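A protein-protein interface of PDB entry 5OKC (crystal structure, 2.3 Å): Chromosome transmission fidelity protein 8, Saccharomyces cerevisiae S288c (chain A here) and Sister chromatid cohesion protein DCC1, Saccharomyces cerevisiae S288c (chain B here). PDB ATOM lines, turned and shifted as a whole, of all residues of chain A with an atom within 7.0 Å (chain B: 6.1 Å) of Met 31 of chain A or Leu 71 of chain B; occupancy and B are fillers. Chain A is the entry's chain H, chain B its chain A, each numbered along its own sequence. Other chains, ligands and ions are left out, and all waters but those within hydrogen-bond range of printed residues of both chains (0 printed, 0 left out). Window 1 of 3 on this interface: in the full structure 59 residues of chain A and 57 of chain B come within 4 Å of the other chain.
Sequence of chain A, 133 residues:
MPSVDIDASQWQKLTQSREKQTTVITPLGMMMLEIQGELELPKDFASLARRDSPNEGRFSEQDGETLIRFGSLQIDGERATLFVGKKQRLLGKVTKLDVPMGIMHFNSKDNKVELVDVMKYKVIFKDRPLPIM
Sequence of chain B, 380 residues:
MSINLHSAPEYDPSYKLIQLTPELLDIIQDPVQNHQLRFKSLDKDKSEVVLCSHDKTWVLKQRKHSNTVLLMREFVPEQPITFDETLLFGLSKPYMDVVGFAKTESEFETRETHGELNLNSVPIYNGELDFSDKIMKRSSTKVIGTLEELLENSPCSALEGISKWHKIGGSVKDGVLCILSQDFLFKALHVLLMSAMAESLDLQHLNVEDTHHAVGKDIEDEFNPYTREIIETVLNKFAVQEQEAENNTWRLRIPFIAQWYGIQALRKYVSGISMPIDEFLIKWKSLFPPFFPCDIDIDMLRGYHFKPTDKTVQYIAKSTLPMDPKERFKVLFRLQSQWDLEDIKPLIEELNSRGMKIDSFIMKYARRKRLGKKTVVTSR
N of Ile 3 of chain B is in hydrogen-bond range of O of Leu 73 of chain A (2.7 Å).
O of Met 104 of chain A lies within hydrogen-bond range of N of Lys 16 of chain B.
The backbone carbonyl oxygen of Leu 33 of chain A lies within hydrogen-bond range of the backbone NH of Leu 70 of chain B (2.9 Å).
N of Met 31 of chain A is in hydrogen-bond range of O of Met 72 of chain B.
The backbone carbonyl oxygen of Lys 16 of chain B lies close to the backbone carbonyl oxygen of Gly 102 of chain A (3.3 Å).
The backbone NH (N) of Thr 104 of chain B lies within hydrogen-bond range of the backbone carbonyl oxygen (O) of Val 69 of chain B (2.9 Å).
The backbone carbonyl oxygen of Leu 71 of chain B sits at hydrogen-bond distance from the backbone NH of Phe 101 of chain B (2.7 Å).
The backbone NH (N) of Leu 71 of chain B sits at hydrogen-bond distance from the backbone carbonyl oxygen (O) of Ala 102 of chain B (2.9 Å).
The backbone NH (N) of Val 99 of chain B is in hydrogen-bond range of the backbone carbonyl oxygen (O) of Arg 73 of chain B (2.8 Å).
N of Gly 29 of chain A sits at hydrogen-bond distance from OG1 of Thr 26 of chain A (3.4 Å).
The backbone NH of Met 30 of chain A is in hydrogen-bond range of the side-chain hydroxyl of Thr 26 of chain A, at 3.1 Å.
CG2 of Ile 25 of chain A touches CE of Met 96 of chain B (3.8 Å).
Arg 73 of chain B touches Gly 29 of chain A (CA to O, 3.3 Å).
Met 72 of chain B touches Met 30 of chain A (O to CA, 3.3 Å).
Leu 17 of chain B touches Met 32 of chain A.
CA of Met 32 of chain A touches O of Leu 70 of chain B, 3.7 Å away.
Met 32 of chain A touches Leu 71 of chain B (CE to CD2, 3.7 Å).
O of Leu 33 of chain A touches CA of Val 69 of chain B, at 3.3 Å.
Gly 102 of chain A touches Leu 17 of chain B (O to CA, 3.5 Å).
Ile 103 of chain A touches Lys 16 of chain B.
Tyr 15 of chain B touches Met 104 of chain A (CA to O, 3.3 Å).
Met 31 of chain A touches three residues of chain B.
Of the printed residues of chain B, Leu 73 of chain A touches Ile 3 and Leu 5.
Of the printed residues of chain A, Ile 3 of chain B touches Leu 73.
Of the printed residues of chain A, Lys 16 of chain B touches Gly 102, Ile 103 and Met 104.
Printed residues of chain A within 4 Å of Leu 71 of chain B: Met 31, Met 32 and Ile 103.
Gly 100 of chain B touches none of the printed residues of chain A.
The nearest printed residue of chain A that does not touch Leu 70 of chain B is Glu 34 of chain A (5.1 Å).
Of the 19 printed residues of chain A, 10 touch a printed residue of chain B.
Hydrophobic or aromatic side chains of chain A that line the printed part of chain B: Ile 25, Met 30, Met 31, Met 32, Leu 33, Leu 73 and Ile 103.
Of the 18 printed residues of chain B, 12 touch a printed residue of chain A.
Hydrophobic or aromatic side chains of chain B within 4 Å of the printed part of chain A: Ile 3, Leu 5, Leu 17, Leu 71, Met 96 and Phe 101.
Among the printed residues, 22 pairs touch across the chains.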
ATOM      1  N   VAL A  24      20.725 -21.057  23.361  1.00  0.00           N
ATOM      2  CA  VAL A  24      19.309 -20.908  23.049  1.00  0.00           C
ATOM      3  C   VAL A  24      18.441 -20.998  24.299  1.00  0.00           C
ATOM      4  O   VAL A  24      17.292 -20.555  24.298  1.00  0.00           O
ATOM      5  CB  VAL A  24      18.851 -21.970  22.033  1.00  0.00           C
ATOM      6  CG1 VAL A  24      19.876 -22.089  20.929  1.00  0.00           C
ATOM      7  CG2 VAL A  24      18.654 -23.319  22.709  1.00  0.00           C
ATOM      8  N   ILE A  25      18.995 -21.582  25.358  1.00  0.00           N
ATOM      9  CA  ILE A  25      18.280 -21.724  26.616  1.00  0.00           C
ATOM     10  C   ILE A  25      17.878 -20.363  27.170  1.00  0.00           C
ATOM     11  O   ILE A  25      18.706 -19.461  27.305  1.00  0.00           O
ATOM     12  CB  ILE A  25      19.135 -22.461  27.666  1.00  0.00           C
ATOM     13  CG1 ILE A  25      19.836 -23.666  27.038  1.00  0.00           C
ATOM     14  CG2 ILE A  25      18.282 -22.884  28.852  1.00  0.00           C
ATOM     15  CD1 ILE A  25      18.893 -24.761  26.611  1.00  0.00           C
ATOM     16  N   THR A  26      16.594 -20.226  27.481  1.00  0.00           N
ATOM     17  CA  THR A  26      16.058 -18.995  28.048  1.00  0.00           C
ATOM     18  C   THR A  26      16.637 -18.752  29.438  1.00  0.00           C
ATOM     19  O   THR A  26      17.120 -19.686  30.077  1.00  0.00           O
ATOM     20  CB  THR A  26      14.513 -19.041  28.125  1.00  0.00           C
ATOM     21  OG1 THR A  26      14.107 -20.018  29.092  1.00  0.00           O
ATOM     22  CG2 THR A  26      13.921 -19.394  26.770  1.00  0.00           C
ATOM     23  N   GLY A  29      15.605 -21.064  31.900  1.00  0.00           N
ATOM     24  CA  GLY A  29      16.161 -22.400  31.790  1.00  0.00           C
ATOM     25  C   GLY A  29      15.324 -23.384  30.995  1.00  0.00           C
ATOM     26  O   GLY A  29      15.208 -24.549  31.374  1.00  0.00           O
ATOM     27  N   MET A  30      14.747 -22.930  29.887  1.00  0.00           N
ATOM     28  CA  MET A  30      13.893 -23.796  29.082  1.00  0.00           C
ATOM     29  C   MET A  30      14.240 -23.759  27.598  1.00  0.00           C
ATOM     30  O   MET A  30      14.826 -22.794  27.106  1.00  0.00           O
ATOM     31  CB  MET A  30      12.427 -23.421  29.289  1.00  0.00           C
ATOM     32  CG  MET A  30      11.850 -23.967  30.581  1.00  0.00           C
ATOM     33  SD  MET A  30      10.029 -23.384  30.935  1.00  0.00           S
ATOM     34  CE  MET A  30      10.424 -21.817  32.028  1.00  0.00           C
ATOM     35  N   MET A  31      13.876 -24.825  26.891  1.00  0.00           N
ATOM     36  CA  MET A  31      14.163 -24.934  25.466  1.00  0.00           C
ATOM     37  C   MET A  31      13.133 -25.797  24.746  1.00  0.00           C
ATOM     38  O   MET A  31      12.385 -26.549  25.373  1.00  0.00           O
ATOM     39  CB  MET A  31      15.563 -25.504  25.239  1.00  0.00           C
ATOM     40  CG  MET A  31      15.796 -26.859  25.882  1.00  0.00           C
ATOM     41  SD  MET A  31      17.429 -27.719  25.243  1.00  0.00           S
ATOM     42  CE  MET A  31      16.938 -27.919  23.368  1.00  0.00           C
ATOM     43  N   MET A  32      13.114 -25.688  23.422  1.00  0.00           N
ATOM     44  CA  MET A  32      12.166 -26.419  22.593  1.00  0.00           C
ATOM     45  C   MET A  32      12.887 -27.341  21.617  1.00  0.00           C
ATOM     46  O   MET A  32      13.695 -26.893  20.805  1.00  0.00           O
ATOM     47  CB  MET A  32      11.268 -25.443  21.833  1.00  0.00           C
ATOM     48  CG  MET A  32      10.351 -26.083  20.809  1.00  0.00           C
ATOM     49  SD  MET A  32       9.142 -24.761  20.029  1.00  0.00           S
ATOM     50  CE  MET A  32       8.336 -24.112  21.669  1.00  0.00           C
ATOM     51  N   LEU A  33      12.592 -28.632  21.705  1.00  0.00           N
ATOM     52  CA  LEU A  33      13.186 -29.621  20.815  1.00  0.00           C
ATOM     53  C   LEU A  33      12.159 -30.139  19.815  1.00  0.00           C
ATOM     54  O   LEU A  33      11.034 -30.476  20.189  1.00  0.00           O
ATOM     55  CB  LEU A  33      13.768 -30.782  21.621  1.00  0.00           C
ATOM     56  CG  LEU A  33      14.279 -31.987  20.828  1.00  0.00           C
ATOM     57  CD1 LEU A  33      15.447 -31.591  19.941  1.00  0.00           C
ATOM     58  CD2 LEU A  33      14.667 -33.121  21.764  1.00  0.00           C
ATOM     59  N   GLU A  34      12.537 -30.191  18.542  1.00  0.00           N
ATOM     60  CA  GLU A  34      11.632 -30.690  17.514  1.00  0.00           C
ATOM     61  C   GLU A  34      12.290 -31.760  16.652  1.00  0.00           C
ATOM     62  O   GLU A  34      13.394 -31.575  16.140  1.00  0.00           O
ATOM     63  CB  GLU A  34      11.134 -29.545  16.631  1.00  0.00           C
ATOM     64  CG  GLU A  34      10.126 -29.985  15.582  1.00  0.00           C
ATOM     65  CD  GLU A  34       9.360 -28.827  14.978  1.00  0.00           C
ATOM     66  OE1 GLU A  34       9.533 -27.684  15.453  1.00  0.00           O
ATOM     67  OE2 GLU A  34       8.582 -29.060  14.029  1.00  0.00           O
ATOM     68  N   LEU A  73      22.592 -33.783  23.534  1.00  0.00           N
ATOM     69  CA  LEU A  73      22.505 -32.694  22.572  1.00  0.00           C
ATOM     70  C   LEU A  73      23.787 -31.875  22.544  1.00  0.00           C
ATOM     71  O   LEU A  73      24.307 -31.483  23.586  1.00  0.00           O
ATOM     72  CB  LEU A  73      21.311 -31.794  22.890  1.00  0.00           C
ATOM     73  CG  LEU A  73      21.101 -30.604  21.953  1.00  0.00           C
ATOM     74  CD1 LEU A  73      20.867 -31.082  20.530  1.00  0.00           C
ATOM     75  CD2 LEU A  73      19.940 -29.751  22.428  1.00  0.00           C
ATOM     76  N   ILE A  75      25.461 -28.478  20.739  1.00  0.00           N
ATOM     77  CA  ILE A  75      25.209 -27.280  19.948  1.00  0.00           C
ATOM     78  C   ILE A  75      26.500 -26.616  19.478  1.00  0.00           C
ATOM     79  O   ILE A  75      27.310 -26.161  20.285  1.00  0.00           O
ATOM     80  CB  ILE A  75      24.383 -26.250  20.740  1.00  0.00           C
ATOM     81  CG1 ILE A  75      23.125 -26.906  21.312  1.00  0.00           C
ATOM     82  CG2 ILE A  75      24.021 -25.068  19.856  1.00  0.00           C
ATOM     83  CD1 ILE A  75      22.221 -27.507  20.260  1.00  0.00           C
ATOM     84  N   GLY A 102       4.595 -18.578  23.114  1.00  0.00           N
ATOM     85  CA  GLY A 102       4.377 -18.444  24.540  1.00  0.00           C
ATOM     86  C   GLY A 102       3.972 -19.770  25.153  1.00  0.00           C
ATOM     87  O   GLY A 102       3.016 -20.403  24.707  1.00  0.00           O
ATOM     88  N   ILE A 103       4.710 -20.199  26.169  1.00  0.00           N
ATOM     89  CA  ILE A 103       4.332 -21.382  26.926  1.00  0.00           C
ATOM     90  C   ILE A 103       3.456 -20.975  28.098  1.00  0.00           C
ATOM     91  O   ILE A 103       3.874 -20.193  28.951  1.00  0.00           O
ATOM     92  CB  ILE A 103       5.555 -22.150  27.452  1.00  0.00           C
ATOM     93  CG1 ILE A 103       6.514 -22.480  26.307  1.00  0.00           C
ATOM     94  CG2 ILE A 103       5.114 -23.422  28.163  1.00  0.00           C
ATOM     95  CD1 ILE A 103       7.708 -23.302  26.738  1.00  0.00           C
ATOM     96  N   MET A 104       2.238 -21.500  28.133  1.00  0.00           N
ATOM     97  CA  MET A 104       1.296 -21.139  29.181  1.00  0.00           C
ATOM     98  C   MET A 104       0.768 -22.368  29.901  1.00  0.00           C
ATOM     99  O   MET A 104       0.557 -23.415  29.290  1.00  0.00           O
ATOM    100  CB  MET A 104       0.136 -20.330  28.601  1.00  0.00           C
ATOM    101  CG  MET A 104       0.569 -19.041  27.922  1.00  0.00           C
ATOM    102  SD  MET A 104      -0.939 -17.882  27.508  1.00  0.00           S
ATOM    103  CE  MET A 104       0.035 -16.423  26.661  1.00  0.00           C
ATOM    104  N   ASP A 117       6.897 -19.354  29.949  1.00  0.00           N
ATOM    105  CA  ASP A 117       8.077 -18.809  29.288  1.00  0.00           C
ATOM    106  C   ASP A 117       7.764 -18.380  27.859  1.00  0.00           C
ATOM    107  O   ASP A 117       6.683 -18.654  27.339  1.00  0.00           O
ATOM    108  CB  ASP A 117       9.213 -19.835  29.283  1.00  0.00           C
ATOM    109  CG  ASP A 117      10.586 -19.188  29.246  1.00  0.00           C
ATOM    110  OD1 ASP A 117      10.672 -17.993  28.890  1.00  0.00           O
ATOM    111  OD2 ASP A 117      11.578 -19.876  29.567  1.00  0.00           O
ATOM    112  N   MET A 119       9.332 -18.707  24.023  1.00  0.00           N
ATOM    113  CA  MET A 119      10.299 -19.391  23.174  1.00  0.00           C
ATOM    114  C   MET A 119      10.585 -18.599  21.903  1.00  0.00           C
ATOM    115  O   MET A 119       9.674 -18.301  21.132  1.00  0.00           O
ATOM    116  CB  MET A 119       9.793 -20.789  22.818  1.00  0.00           C
ATOM    117  CG  MET A 119       9.508 -21.675  24.021  1.00  0.00           C
ATOM    118  SD  MET A 119      11.125 -22.189  24.979  1.00  0.00           S
ATOM    119  CE  MET A 119      12.292 -22.426  23.446  1.00  0.00           C
ATOM    120  N   TYR A 121      13.591 -19.489  20.050  1.00  0.00           N
ATOM    121  CA  TYR A 121      14.409 -20.387  19.244  1.00  0.00           C
ATOM    122  C   TYR A 121      13.947 -21.824  19.402  1.00  0.00           C
ATOM    123  O   TYR A 121      13.260 -22.160  20.365  1.00  0.00           O
ATOM    124  CB  TYR A 121      15.884 -20.276  19.633  1.00  0.00           C
ATOM    125  CG  TYR A 121      16.496 -18.925  19.359  1.00  0.00           C
ATOM    126  CD1 TYR A 121      16.426 -17.903  20.297  1.00  0.00           C
ATOM    127  CD2 TYR A 121      17.152 -18.672  18.161  1.00  0.00           C
ATOM    128  CE1 TYR A 121      16.987 -16.666  20.047  1.00  0.00           C
ATOM    129  CE2 TYR A 121      17.715 -17.439  17.903  1.00  0.00           C
ATOM    130  CZ  TYR A 121      17.630 -16.439  18.848  1.00  0.00           C
ATOM    131  OH  TYR A 121      18.190 -15.207  18.597  1.00  0.00           O
ATOM    132  N   LYS A 122      14.328 -22.675  18.458  1.00  0.00           N
ATOM    133  CA  LYS A 122      14.092 -24.104  18.611  1.00  0.00           C
ATOM    134  C   LYS A 122      15.216 -24.902  17.965  1.00  0.00           C
ATOM    135  O   LYS A 122      15.823 -24.463  16.988  1.00  0.00           O
ATOM    136  CB  LYS A 122      12.743 -24.509  18.010  1.00  0.00           C
ATOM    137  CG  LYS A 122      12.682 -24.432  16.495  1.00  0.00           C
ATOM    138  CD  LYS A 122      11.382 -25.009  15.957  1.00  0.00           C
ATOM    139  CE  LYS A 122      11.305 -24.886  14.443  1.00  0.00           C
ATOM    140  NZ  LYS A 122      10.017 -25.411  13.905  1.00  0.00           N
ATOM    141  N   VAL A 123      15.493 -26.073  18.527  1.00  0.00           N
ATOM    142  CA  VAL A 123      16.475 -26.984  17.960  1.00  0.00           C
ATOM    143  C   VAL A 123      15.742 -28.086  17.205  1.00  0.00           C
ATOM    144  O   VAL A 123      15.124 -28.960  17.812  1.00  0.00           O
ATOM    145  CB  VAL A 123      17.376 -27.595  19.042  1.00  0.00           C
ATOM    146  CG1 VAL A 123      18.536 -28.337  18.403  1.00  0.00           C
ATOM    147  CG2 VAL A 123      17.892 -26.507  19.970  1.00  0.00           C
ATOM    148  N   ILE B   3      24.579 -31.689  26.219  1.00  0.00           N
ATOM    149  CA  ILE B   3      23.453 -31.593  27.135  1.00  0.00           C
ATOM    150  C   ILE B   3      22.747 -32.938  27.268  1.00  0.00           C
ATOM    151  O   ILE B   3      22.333 -33.532  26.273  1.00  0.00           O
ATOM    152  CB  ILE B   3      22.440 -30.533  26.670  1.00  0.00           C
ATOM    153  CG1 ILE B   3      23.140 -29.189  26.447  1.00  0.00           C
ATOM    154  CG2 ILE B   3      21.316 -30.398  27.682  1.00  0.00           C
ATOM    155  CD1 ILE B   3      22.245 -28.120  25.855  1.00  0.00           C
ATOM    156  N   LEU B   5      19.719 -35.231  27.798  1.00  0.00           N
ATOM    157  CA  LEU B   5      18.284 -35.115  27.583  1.00  0.00           C
ATOM    158  C   LEU B   5      17.525 -36.172  28.372  1.00  0.00           C
ATOM    159  O   LEU B   5      17.730 -37.372  28.181  1.00  0.00           O
ATOM    160  CB  LEU B   5      17.957 -35.230  26.095  1.00  0.00           C
ATOM    161  CG  LEU B   5      18.766 -34.314  25.174  1.00  0.00           C
ATOM    162  CD1 LEU B   5      18.234 -34.395  23.761  1.00  0.00           C
ATOM    163  CD2 LEU B   5      18.751 -32.875  25.669  1.00  0.00           C
ATOM    164  N   TYR B  15       0.382 -27.540  29.832  1.00  0.00           N
ATOM    165  CA  TYR B  15       1.316 -26.669  29.126  1.00  0.00           C
ATOM    166  C   TYR B  15       0.984 -26.623  27.641  1.00  0.00           C
ATOM    167  O   TYR B  15       0.963 -27.654  26.968  1.00  0.00           O
ATOM    168  CB  TYR B  15       2.762 -27.136  29.335  1.00  0.00           C
ATOM    169  CG  TYR B  15       3.216 -27.068  30.776  1.00  0.00           C
ATOM    170  CD1 TYR B  15       3.683 -25.878  31.321  1.00  0.00           C
ATOM    171  CD2 TYR B  15       3.170 -28.191  31.594  1.00  0.00           C
ATOM    172  CE1 TYR B  15       4.093 -25.809  32.642  1.00  0.00           C
ATOM    173  CE2 TYR B  15       3.578 -28.130  32.915  1.00  0.00           C
ATOM    174  CZ  TYR B  15       4.039 -26.938  33.433  1.00  0.00           C
ATOM    175  OH  TYR B  15       4.446 -26.872  34.747  1.00  0.00           O
ATOM    176  N   LYS B  16       0.724 -25.424  27.130  1.00  0.00           N
ATOM    177  CA  LYS B  16       0.348 -25.265  25.732  1.00  0.00           C
ATOM    178  C   LYS B  16       1.115 -24.132  25.067  1.00  0.00           C
ATOM    179  O   LYS B  16       1.515 -23.169  25.722  1.00  0.00           O
ATOM    180  CB  LYS B  16      -1.158 -25.013  25.613  1.00  0.00           C
ATOM    181  CG  LYS B  16      -2.023 -26.183  26.064  1.00  0.00           C
ATOM    182  CD  LYS B  16      -3.503 -25.886  25.872  1.00  0.00           C
ATOM    183  CE  LYS B  16      -4.356 -27.102  26.191  1.00  0.00           C
ATOM    184  NZ  LYS B  16      -4.167 -27.552  27.596  1.00  0.00           N
ATOM    185  N   LEU B  17       1.311 -24.252  23.758  1.00  0.00           N
ATOM    186  CA  LEU B  17       2.040 -23.250  22.993  1.00  0.00           C
ATOM    187  C   LEU B  17       1.092 -22.258  22.329  1.00  0.00           C
ATOM    188  O   LEU B  17       0.183 -22.648  21.599  1.00  0.00           O
ATOM    189  CB  LEU B  17       2.918 -23.917  21.935  1.00  0.00           C
ATOM    190  CG  LEU B  17       4.148 -24.663  22.450  1.00  0.00           C
ATOM    191  CD1 LEU B  17       4.899 -25.309  21.298  1.00  0.00           C
ATOM    192  CD2 LEU B  17       5.050 -23.714  23.221  1.00  0.00           C
ATOM    193  N   VAL B  69       7.367 -32.550  19.378  1.00  0.00           N
ATOM    194  CA  VAL B  69       7.819 -31.314  20.001  1.00  0.00           C
ATOM    195  C   VAL B  69       7.865 -31.458  21.516  1.00  0.00           C
ATOM    196  O   VAL B  69       6.837 -31.655  22.170  1.00  0.00           O
ATOM    197  CB  VAL B  69       6.919 -30.124  19.630  1.00  0.00           C
ATOM    198  CG1 VAL B  69       7.311 -28.896  20.438  1.00  0.00           C
ATOM    199  CG2 VAL B  69       7.018 -29.837  18.142  1.00  0.00           C
ATOM    200  N   LEU B  70       9.072 -31.352  22.062  1.00  0.00           N
ATOM    201  CA  LEU B  70       9.287 -31.487  23.495  1.00  0.00           C
ATOM    202  C   LEU B  70       9.668 -30.160  24.137  1.00  0.00           C
ATOM    203  O   LEU B  70      10.654 -29.532  23.756  1.00  0.00           O
ATOM    204  CB  LEU B  70      10.371 -32.527  23.780  1.00  0.00           C
ATOM    205  CG  LEU B  70       9.981 -33.992  23.589  1.00  0.00           C
ATOM    206  CD1 LEU B  70      11.155 -34.898  23.937  1.00  0.00           C
ATOM    207  CD2 LEU B  70       8.762 -34.334  24.435  1.00  0.00           C
ATOM    208  N   LEU B  71       8.869 -29.743  25.110  1.00  0.00           N
ATOM    209  CA  LEU B  71       9.194 -28.603  25.945  1.00  0.00           C
ATOM    210  C   LEU B  71       9.988 -29.107  27.141  1.00  0.00           C
ATOM    211  O   LEU B  71       9.486 -29.915  27.941  1.00  0.00           O
ATOM    212  CB  LEU B  71       7.929 -27.875  26.397  1.00  0.00           C
ATOM    213  CG  LEU B  71       6.952 -27.485  25.286  1.00  0.00           C
ATOM    214  CD1 LEU B  71       5.785 -26.688  25.852  1.00  0.00           C
ATOM    215  CD2 LEU B  71       7.659 -26.708  24.186  1.00  0.00           C
ATOM    216  N   MET B  72      11.229 -28.633  27.238  1.00  0.00           N
ATOM    217  CA  MET B  72      12.189 -29.126  28.220  1.00  0.00           C
ATOM    218  C   MET B  72      12.742 -28.008  29.100  1.00  0.00           C
ATOM    219  O   MET B  72      12.963 -26.890  28.635  1.00  0.00           O
ATOM    220  CB  MET B  72      13.346 -29.846  27.518  1.00  0.00           C
ATOM    221  CG  MET B  72      12.937 -30.655  26.294  1.00  0.00           C
ATOM    222  SD  MET B  72      14.395 -31.743  25.592  1.00  0.00           S
ATOM    223  CE  MET B  72      14.490 -33.059  27.019  1.00  0.00           C
ATOM    224  N   ARG B  73      12.973 -28.324  30.371  1.00  0.00           N
ATOM    225  CA  ARG B  73      13.542 -27.368  31.313  1.00  0.00           C
ATOM    226  C   ARG B  73      14.791 -27.924  31.991  1.00  0.00           C
ATOM    227  O   ARG B  73      14.920 -29.135  32.178  1.00  0.00           O
ATOM    228  CB  ARG B  73      12.512 -26.981  32.376  1.00  0.00           C
ATOM    229  CG  ARG B  73      11.950 -28.159  33.154  1.00  0.00           C
ATOM    230  CD  ARG B  73      11.160 -27.697  34.368  1.00  0.00           C
ATOM    231  NE  ARG B  73      10.446 -28.801  35.002  1.00  0.00           N
ATOM    232  CZ  ARG B  73       9.136 -29.003  34.894  1.00  0.00           C
ATOM    233  NH1 ARG B  73       8.390 -28.169  34.183  1.00  0.00           N
ATOM    234  NH2 ARG B  73       8.571 -30.038  35.503  1.00  0.00           N
ATOM    235  N   MET B  96      25.129 -30.163  31.503  1.00  0.00           N
ATOM    236  CA  MET B  96      23.780 -29.692  31.781  1.00  0.00           C
ATOM    237  C   MET B  96      22.740 -30.785  31.552  1.00  0.00           C
ATOM    238  O   MET B  96      22.848 -31.574  30.613  1.00  0.00           O
ATOM    239  CB  MET B  96      23.475 -28.470  30.909  1.00  0.00           C
ATOM    240  CG  MET B  96      22.086 -27.877  31.066  1.00  0.00           C
ATOM    241  SD  MET B  96      21.906 -26.247  30.004  1.00  0.00           S
ATOM    242  CE  MET B  96      20.010 -25.903  30.265  1.00  0.00           C
ATOM    243  N   VAL B  98      18.565 -31.434  31.066  1.00  0.00           N
ATOM    244  CA  VAL B  98      17.216 -30.917  30.876  1.00  0.00           C
ATOM    245  C   VAL B  98      16.214 -32.063  30.817  1.00  0.00           C
ATOM    246  O   VAL B  98      16.542 -33.170  30.384  1.00  0.00           O
ATOM    247  CB  VAL B  98      17.100 -30.062  29.596  1.00  0.00           C
ATOM    248  CG1 VAL B  98      18.046 -28.874  29.663  1.00  0.00           C
ATOM    249  CG2 VAL B  98      17.376 -30.896  28.359  1.00  0.00           C
ATOM    250  N   VAL B  99      14.993 -31.798  31.270  1.00  0.00           N
ATOM    251  CA  VAL B  99      13.940 -32.804  31.234  1.00  0.00           C
ATOM    252  C   VAL B  99      12.740 -32.309  30.436  1.00  0.00           C
ATOM    253  O   VAL B  99      12.258 -31.195  30.641  1.00  0.00           O
ATOM    254  CB  VAL B  99      13.487 -33.208  32.661  1.00  0.00           C
ATOM    255  CG1 VAL B  99      13.134 -31.982  33.499  1.00  0.00           C
ATOM    256  CG2 VAL B  99      12.317 -34.182  32.594  1.00  0.00           C
ATOM    257  N   GLY B 100      12.272 -33.136  29.508  1.00  0.00           N
ATOM    258  CA  GLY B 100      11.080 -32.811  28.755  1.00  0.00           C
ATOM    259  C   GLY B 100       9.883 -32.887  29.678  1.00  0.00           C
ATOM    260  O   GLY B 100       9.511 -33.969  30.132  1.00  0.00           O
ATOM    261  N   PHE B 101       9.280 -31.737  29.958  1.00  0.00           N
ATOM    262  CA  PHE B 101       8.124 -31.692  30.841  1.00  0.00           C
ATOM    263  C   PHE B 101       6.835 -31.616  30.038  1.00  0.00           C
ATOM    264  O   PHE B 101       5.750 -31.853  30.571  1.00  0.00           O
ATOM    265  CB  PHE B 101       8.217 -30.505  31.806  1.00  0.00           C
ATOM    266  CG  PHE B 101       8.204 -29.164  31.128  1.00  0.00           C
ATOM    267  CD1 PHE B 101       9.381 -28.584  30.685  1.00  0.00           C
ATOM    268  CD2 PHE B 101       7.013 -28.481  30.938  1.00  0.00           C
ATOM    269  CE1 PHE B 101       9.370 -27.350  30.062  1.00  0.00           C
ATOM    270  CE2 PHE B 101       6.997 -27.248  30.315  1.00  0.00           C
ATOM    271  CZ  PHE B 101       8.176 -26.682  29.878  1.00  0.00           C
ATOM    272  N   ALA B 102       6.947 -31.293  28.752  1.00  0.00           N
ATOM    273  CA  ALA B 102       5.751 -31.259  27.916  1.00  0.00           C
ATOM    274  C   ALA B 102       5.992 -31.849  26.530  1.00  0.00           C
ATOM    275  O   ALA B 102       7.100 -31.800  26.008  1.00  0.00           O
ATOM    276  CB  ALA B 102       5.234 -29.833  27.795  1.00  0.00           C
ATOM    277  N   LYS B 103       4.950 -32.438  25.955  1.00  0.00           N
ATOM    278  CA  LYS B 103       5.011 -32.928  24.583  1.00  0.00           C
ATOM    279  C   LYS B 103       3.807 -32.425  23.797  1.00  0.00           C
ATOM    280  O   LYS B 103       2.698 -32.935  23.955  1.00  0.00           O
ATOM    281  CB  LYS B 103       5.069 -34.454  24.538  1.00  0.00           C
ATOM    282  CG  LYS B 103       5.189 -35.007  23.126  1.00  0.00           C
ATOM    283  CD  LYS B 103       5.053 -36.517  23.094  1.00  0.00           C
ATOM    284  CE  LYS B 103       5.116 -37.038  21.666  1.00  0.00           C
ATOM    285  NZ  LYS B 103       4.025 -36.487  20.814  1.00  0.00           N
ATOM    286  N   THR B 104       4.024 -31.426  22.948  1.00  0.00           N
ATOM    287  CA  THR B 104       2.916 -30.803  22.235  1.00  0.00           C
ATOM    288  C   THR B 104       2.789 -31.330  20.812  1.00  0.00           C
ATOM    289  O   THR B 104       3.786 -31.541  20.123  1.00  0.00           O
ATOM    290  CB  THR B 104       3.061 -29.271  22.193  1.00  0.00           C
ATOM    291  OG1 THR B 104       4.282 -28.920  21.529  1.00  0.00           O
ATOM    292  CG2 THR B 104       3.074 -28.701  23.601  1.00  0.00           C
